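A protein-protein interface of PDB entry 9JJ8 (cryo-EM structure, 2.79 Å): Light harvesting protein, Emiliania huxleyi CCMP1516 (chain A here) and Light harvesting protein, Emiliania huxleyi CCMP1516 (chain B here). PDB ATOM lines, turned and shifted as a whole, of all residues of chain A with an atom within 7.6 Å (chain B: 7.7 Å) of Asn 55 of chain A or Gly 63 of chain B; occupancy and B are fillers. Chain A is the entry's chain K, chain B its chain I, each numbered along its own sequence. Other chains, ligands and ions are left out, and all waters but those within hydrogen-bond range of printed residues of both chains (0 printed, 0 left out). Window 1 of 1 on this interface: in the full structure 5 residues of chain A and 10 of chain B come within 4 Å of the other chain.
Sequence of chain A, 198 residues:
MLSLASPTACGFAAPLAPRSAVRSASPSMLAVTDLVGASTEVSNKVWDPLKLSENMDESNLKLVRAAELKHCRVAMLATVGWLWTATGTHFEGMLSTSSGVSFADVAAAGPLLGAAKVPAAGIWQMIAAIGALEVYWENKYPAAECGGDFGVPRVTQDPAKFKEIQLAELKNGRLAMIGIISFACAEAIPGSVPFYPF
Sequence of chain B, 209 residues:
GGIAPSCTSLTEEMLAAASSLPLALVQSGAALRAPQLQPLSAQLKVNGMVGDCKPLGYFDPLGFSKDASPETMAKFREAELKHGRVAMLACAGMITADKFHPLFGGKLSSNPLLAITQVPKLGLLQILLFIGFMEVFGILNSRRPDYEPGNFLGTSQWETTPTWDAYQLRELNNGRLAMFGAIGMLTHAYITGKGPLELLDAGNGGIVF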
ATOM      1  N   ASP A  48       4.375  18.234  28.320  1.00  0.00           N
ATOM      2  CA  ASP A  48       2.969  17.827  28.288  1.00  0.00           C
ATOM      3  C   ASP A  48       2.690  17.146  26.956  1.00  0.00           C
ATOM      4  O   ASP A  48       2.137  17.752  26.031  1.00  0.00           O
ATOM      5  CB  ASP A  48       2.047  19.028  28.509  1.00  0.00           C
ATOM      6  CG  ASP A  48       0.717  18.634  29.118  1.00  0.00           C
ATOM      7  OD1 ASP A  48       0.589  17.477  29.570  1.00  0.00           O
ATOM      8  OD2 ASP A  48      -0.197  19.483  29.150  1.00  0.00           O
ATOM      9  N   LYS A  51      -0.963  16.895  26.256  1.00  0.00           N
ATOM     10  CA  LYS A  51      -1.580  18.228  26.252  1.00  0.00           C
ATOM     11  C   LYS A  51      -2.717  18.328  27.267  1.00  0.00           C
ATOM     12  O   LYS A  51      -3.786  18.872  26.986  1.00  0.00           O
ATOM     13  CB  LYS A  51      -2.057  18.615  24.850  1.00  0.00           C
ATOM     14  CG  LYS A  51      -0.965  19.182  23.951  1.00  0.00           C
ATOM     15  CD  LYS A  51      -0.227  18.080  23.203  1.00  0.00           C
ATOM     16  CE  LYS A  51       0.936  18.635  22.397  1.00  0.00           C
ATOM     17  NZ  LYS A  51       1.684  17.559  21.690  1.00  0.00           N
ATOM     18  N   LEU A  52      -2.479  17.785  28.465  1.00  0.00           N
ATOM     19  CA  LEU A  52      -3.486  17.812  29.520  1.00  0.00           C
ATOM     20  C   LEU A  52      -3.739  19.218  30.045  1.00  0.00           C
ATOM     21  O   LEU A  52      -4.831  19.491  30.554  1.00  0.00           O
ATOM     22  CB  LEU A  52      -3.061  16.896  30.670  1.00  0.00           C
ATOM     23  CG  LEU A  52      -3.098  15.389  30.404  1.00  0.00           C
ATOM     24  CD1 LEU A  52      -2.645  14.614  31.629  1.00  0.00           C
ATOM     25  CD2 LEU A  52      -4.487  14.947  29.975  1.00  0.00           C
ATOM     26  N   SER A  53      -2.761  20.114  29.931  1.00  0.00           N
ATOM     27  CA  SER A  53      -2.887  21.484  30.409  1.00  0.00           C
ATOM     28  C   SER A  53      -3.115  22.480  29.279  1.00  0.00           C
ATOM     29  O   SER A  53      -2.902  23.681  29.476  1.00  0.00           O
ATOM     30  CB  SER A  53      -1.646  21.879  31.212  1.00  0.00           C
ATOM     31  OG  SER A  53      -0.475  21.769  30.423  1.00  0.00           O
ATOM     32  N   GLU A  54      -3.528  22.008  28.099  1.00  0.00           N
ATOM     33  CA  GLU A  54      -3.758  22.908  26.973  1.00  0.00           C
ATOM     34  C   GLU A  54      -4.945  23.827  27.228  1.00  0.00           C
ATOM     35  O   GLU A  54      -4.868  25.038  26.984  1.00  0.00           O
ATOM     36  CB  GLU A  54      -3.974  22.099  25.694  1.00  0.00           C
ATOM     37  CG  GLU A  54      -4.299  22.941  24.472  1.00  0.00           C
ATOM     38  CD  GLU A  54      -4.735  22.105  23.283  1.00  0.00           C
ATOM     39  OE1 GLU A  54      -4.700  20.861  23.384  1.00  0.00           O
ATOM     40  OE2 GLU A  54      -5.113  22.693  22.249  1.00  0.00           O
ATOM     41  N   ASN A  55      -6.051  23.275  27.729  1.00  0.00           N
ATOM     42  CA  ASN A  55      -7.275  24.028  28.005  1.00  0.00           C
ATOM     43  C   ASN A  55      -7.715  23.719  29.434  1.00  0.00           C
ATOM     44  O   ASN A  55      -8.594  22.882  29.658  1.00  0.00           O
ATOM     45  CB  ASN A  55      -8.362  23.681  26.979  1.00  0.00           C
ATOM     46  CG  ASN A  55      -8.472  22.183  26.719  1.00  0.00           C
ATOM     47  OD1 ASN A  55      -7.762  21.381  27.326  1.00  0.00           O
ATOM     48  ND2 ASN A  55      -9.376  21.802  25.825  1.00  0.00           N
ATOM     49  N   MET A  56      -7.125  24.408  30.413  1.00  0.00           N
ATOM     50  CA  MET A  56      -7.402  24.036  31.795  1.00  0.00           C
ATOM     51  C   MET A  56      -7.716  25.247  32.674  1.00  0.00           C
ATOM     52  O   MET A  56      -8.399  25.094  33.695  1.00  0.00           O
ATOM     53  CB  MET A  56      -6.216  23.224  32.338  1.00  0.00           C
ATOM     54  CG  MET A  56      -6.345  22.686  33.759  1.00  0.00           C
ATOM     55  SD  MET A  56      -4.789  21.990  34.350  1.00  0.00           S
ATOM     56  CE  MET A  56      -4.991  20.262  33.917  1.00  0.00           C
ATOM     57  N   ASP A  57      -7.233  26.442  32.289  1.00  0.00           N
ATOM     58  CA  ASP A  57      -7.527  27.736  32.926  1.00  0.00           C
ATOM     59  C   ASP A  57      -6.932  27.823  34.337  1.00  0.00           C
ATOM     60  O   ASP A  57      -6.537  26.812  34.925  1.00  0.00           O
ATOM     61  CB  ASP A  57      -9.054  27.991  32.929  1.00  0.00           C
ATOM     62  CG  ASP A  57      -9.452  29.405  33.376  1.00  0.00           C
ATOM     63  OD1 ASP A  57      -8.581  30.229  33.726  1.00  0.00           O
ATOM     64  OD2 ASP A  57     -10.671  29.682  33.391  1.00  0.00           O
ATOM     65  N   ASN A  60      -7.691  25.821  38.202  1.00  0.00           N
ATOM     66  CA  ASN A  60      -7.496  24.398  37.949  1.00  0.00           C
ATOM     67  C   ASN A  60      -6.033  24.072  37.704  1.00  0.00           C
ATOM     68  O   ASN A  60      -5.565  23.012  38.124  1.00  0.00           O
ATOM     69  CB  ASN A  60      -8.333  23.934  36.745  1.00  0.00           C
ATOM     70  CG  ASN A  60      -9.823  23.999  37.007  1.00  0.00           C
ATOM     71  OD1 ASN A  60     -10.568  24.630  36.259  1.00  0.00           O
ATOM     72  ND2 ASN A  60     -10.266  23.337  38.068  1.00  0.00           N
ATOM     73  N   ASP B  60     -13.119  21.835  36.151  1.00  0.00           N
ATOM     74  CA  ASP B  60     -13.133  21.545  34.720  1.00  0.00           C
ATOM     75  C   ASP B  60     -11.721  21.591  34.144  1.00  0.00           C
ATOM     76  O   ASP B  60     -11.354  22.548  33.452  1.00  0.00           O
ATOM     77  CB  ASP B  60     -14.052  22.512  33.975  1.00  0.00           C
ATOM     78  CG  ASP B  60     -14.397  22.024  32.585  1.00  0.00           C
ATOM     79  OD1 ASP B  60     -14.512  20.795  32.398  1.00  0.00           O
ATOM     80  OD2 ASP B  60     -14.542  22.867  31.678  1.00  0.00           O
ATOM     81  N   PRO B  61     -10.900  20.573  34.408  1.00  0.00           N
ATOM     82  CA  PRO B  61      -9.779  20.311  33.507  1.00  0.00           C
ATOM     83  C   PRO B  61     -10.294  19.596  32.270  1.00  0.00           C
ATOM     84  O   PRO B  61     -11.451  19.173  32.211  1.00  0.00           O
ATOM     85  CB  PRO B  61      -8.851  19.422  34.336  1.00  0.00           C
ATOM     86  CG  PRO B  61      -9.762  18.694  35.236  1.00  0.00           C
ATOM     87  CD  PRO B  61     -10.912  19.618  35.533  1.00  0.00           C
ATOM     88  N   LEU B  62      -9.431  19.518  31.254  1.00  0.00           N
ATOM     89  CA  LEU B  62      -9.688  18.980  29.914  1.00  0.00           C
ATOM     90  C   LEU B  62     -10.668  19.826  29.107  1.00  0.00           C
ATOM     91  O   LEU B  62     -10.924  19.497  27.942  1.00  0.00           O
ATOM     92  CB  LEU B  62     -10.192  17.525  29.924  1.00  0.00           C
ATOM     93  CG  LEU B  62      -9.195  16.365  29.899  1.00  0.00           C
ATOM     94  CD1 LEU B  62      -8.270  16.402  31.091  1.00  0.00           C
ATOM     95  CD2 LEU B  62      -9.948  15.044  29.859  1.00  0.00           C
ATOM     96  N   GLY B  63     -11.216  20.897  29.673  1.00  0.00           N
ATOM     97  CA  GLY B  63     -12.044  21.833  28.928  1.00  0.00           C
ATOM     98  C   GLY B  63     -13.339  21.270  28.384  1.00  0.00           C
ATOM     99  O   GLY B  63     -13.685  21.533  27.226  1.00  0.00           O
ATOM    100  N   PHE B  64     -14.061  20.488  29.188  1.00  0.00           N
ATOM    101  CA  PHE B  64     -15.344  19.972  28.725  1.00  0.00           C
ATOM    102  C   PHE B  64     -16.401  21.067  28.676  1.00  0.00           C
ATOM    103  O   PHE B  64     -17.326  20.998  27.860  1.00  0.00           O
ATOM    104  CB  PHE B  64     -15.810  18.824  29.618  1.00  0.00           C
ATOM    105  CG  PHE B  64     -15.247  17.486  29.230  1.00  0.00           C
ATOM    106  CD1 PHE B  64     -15.591  16.896  28.025  1.00  0.00           C
ATOM    107  CD2 PHE B  64     -14.379  16.815  30.075  1.00  0.00           C
ATOM    108  CE1 PHE B  64     -15.073  15.663  27.667  1.00  0.00           C
ATOM    109  CE2 PHE B  64     -13.860  15.581  29.726  1.00  0.00           C
ATOM    110  CZ  PHE B  64     -14.206  15.004  28.519  1.00  0.00           C
ATOM    111  N   SER B  65     -16.281  22.082  29.529  1.00  0.00           N
ATOM    112  CA  SER B  65     -17.271  23.143  29.604  1.00  0.00           C
ATOM    113  C   SER B  65     -16.793  24.471  29.035  1.00  0.00           C
ATOM    114  O   SER B  65     -17.539  25.453  29.098  1.00  0.00           O
ATOM    115  CB  SER B  65     -17.722  23.339  31.055  1.00  0.00           C
ATOM    116  OG  SER B  65     -18.448  24.546  31.202  1.00  0.00           O
ATOM    117  N   LYS B  66     -15.578  24.539  28.488  1.00  0.00           N
ATOM    118  CA  LYS B  66     -15.125  25.754  27.821  1.00  0.00           C
ATOM    119  C   LYS B  66     -15.800  25.828  26.456  1.00  0.00           C
ATOM    120  O   LYS B  66     -15.863  24.825  25.736  1.00  0.00           O
ATOM    121  CB  LYS B  66     -13.589  25.804  27.718  1.00  0.00           C
ATOM    122  CG  LYS B  66     -12.858  24.737  26.865  1.00  0.00           C
ATOM    123  CD  LYS B  66     -12.656  25.141  25.396  1.00  0.00           C
ATOM    124  CE  LYS B  66     -11.843  24.101  24.632  1.00  0.00           C
ATOM    125  NZ  LYS B  66     -11.633  24.432  23.181  1.00  0.00           N
ATOM    126  N   ASP B  67     -16.371  26.996  26.153  1.00  0.00           N
ATOM    127  CA  ASP B  67     -16.984  27.336  24.862  1.00  0.00           C
ATOM    128  C   ASP B  67     -18.008  26.292  24.411  1.00  0.00           C
ATOM    129  O   ASP B  67     -17.942  25.737  23.312  1.00  0.00           O
ATOM    130  CB  ASP B  67     -15.913  27.564  23.795  1.00  0.00           C
ATOM    131  CG  ASP B  67     -15.108  28.824  24.049  1.00  0.00           C
ATOM    132  OD1 ASP B  67     -15.658  29.773  24.650  1.00  0.00           O
ATOM    133  OD2 ASP B  67     -13.930  28.872  23.640  1.00  0.00           O
ATOM    134  N   ALA B  68     -18.976  26.048  25.284  1.00  0.00           N
ATOM    135  CA  ALA B  68     -20.004  25.050  25.047  1.00  0.00           C
ATOM    136  C   ALA B  68     -21.370  25.683  25.238  1.00  0.00           C
ATOM    137  O   ALA B  68     -21.540  26.575  26.075  1.00  0.00           O
ATOM    138  CB  ALA B  68     -19.836  23.848  25.980  1.00  0.00           C
ATOM    139  N   MET B  73     -24.472  22.055  28.558  1.00  0.00           N
ATOM    140  CA  MET B  73     -24.412  22.140  30.015  1.00  0.00           C
ATOM    141  C   MET B  73     -25.619  21.479  30.665  1.00  0.00           C
ATOM    142  O   MET B  73     -25.485  20.805  31.693  1.00  0.00           O
ATOM    143  CB  MET B  73     -24.301  23.603  30.448  1.00  0.00           C
ATOM    144  CG  MET B  73     -23.011  24.301  30.027  1.00  0.00           C
ATOM    145  SD  MET B  73     -21.517  23.562  30.720  1.00  0.00           S
ATOM    146  CE  MET B  73     -20.898  22.635  29.317  1.00  0.00           C
ATOM    147  N   PHE B  76     -25.076  17.725  30.375  1.00  0.00           N
ATOM    148  CA  PHE B  76     -24.062  17.269  31.321  1.00  0.00           C
ATOM    149  C   PHE B  76     -24.594  17.255  32.750  1.00  0.00           C
ATOM    150  O   PHE B  76     -24.316  16.321  33.513  1.00  0.00           O
ATOM    151  CB  PHE B  76     -22.814  18.149  31.225  1.00  0.00           C
ATOM    152  CG  PHE B  76     -21.953  17.866  30.024  1.00  0.00           C
ATOM    153  CD1 PHE B  76     -22.107  16.697  29.297  1.00  0.00           C
ATOM    154  CD2 PHE B  76     -20.970  18.763  29.639  1.00  0.00           C
ATOM    155  CE1 PHE B  76     -21.310  16.439  28.197  1.00  0.00           C
ATOM    156  CE2 PHE B  76     -20.167  18.508  28.543  1.00  0.00           C
ATOM    157  CZ  PHE B  76     -20.339  17.343  27.820  1.00  0.00           C
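The side-chain amide nitrogen (ND2) of Asn 55 of chain A lies within hydrogen-bond range of the backbone carbonyl oxygen (O) of Leu 62 of chain B (3.5 Å).
The backbone carbonyl oxygen (O) of Asn 55 of chain A is in hydrogen-bond range of the backbone NH (N) of Gly 63 of chain B, 3.3 Å away.
O of Met 56 of chain A lies close to OD1 of Asn 60 of chain A, at 3.4 Å.
The side-chain carboxylate of Asp 60 of chain B lies within hydrogen-bond range of the backbone NH of Phe 64 of chain B, at 3.3 Å.
OD2 of Asp 60 of chain B sits at hydrogen-bond distance from N of Ser 65 of chain B (2.9 Å).
Among the printed residues, pairs that only touch across the chains: Asn 55 of chain A with Lys 66 of chain B (3.6 Å), Met 56 of chain A with Asp 60 of chain B (3.9 Å), Met 56 of chain A with Pro 61 of chain B (3.97 Å) and Asn 60 of chain A with Asp 60 of chain B (3.6 Å).
Asn 55 of chain A touches just these residues of chain B: Leu 62 (3.5 Å), Gly 63 (3.3 Å) and Lys 66 (3.6 Å).
Of chain A, only Asn 55 (3.3 Å) comes within 4 Å of Gly 63 of chain B.
Of the printed residues of chain B, Asn 60 of chain A touches Asp 60 (3.6 Å).
Of the printed residues of chain A, Pro 61 of chain B touches Met 56 (3.97 Å).
Of the printed residues of chain B, Met 56 of chain A touches Asp 60 and Pro 61.
Printed residues of chain A within 4 Å of Lys 66 of chain B: Asn 55 (3.6 Å).
Of the printed residues of chain A, Leu 62 of chain B touches Asn 55 (3.5 Å).
Ser 53 of chain A touches none of the printed residues of chain B.
The nearest residue of chain B that does not touch Asn 55 of chain A is Pro 61 of chain B (4.5 Å).
The nearest printed residue of chain A that does not touch Asp 60 of chain B is Asn 55 of chain A (4.7 Å).
Of the 9 printed residues of chain A, 3 touch a printed residue of chain B.
Printed residues of chain A that touch a printed residue of chain B: Asn 55, Met 56 and Asn 60.
Of the 11 printed residues of chain B, 5 touch a printed residue of chain A.
Hydrophobic or aromatic side chains of chain B that line the printed part of chain A: Pro 61.
Among the printed residues, no Asp or Glu carboxylate lies within 4 Å of a Lys or Arg side-chain nitrogen of the other chain.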
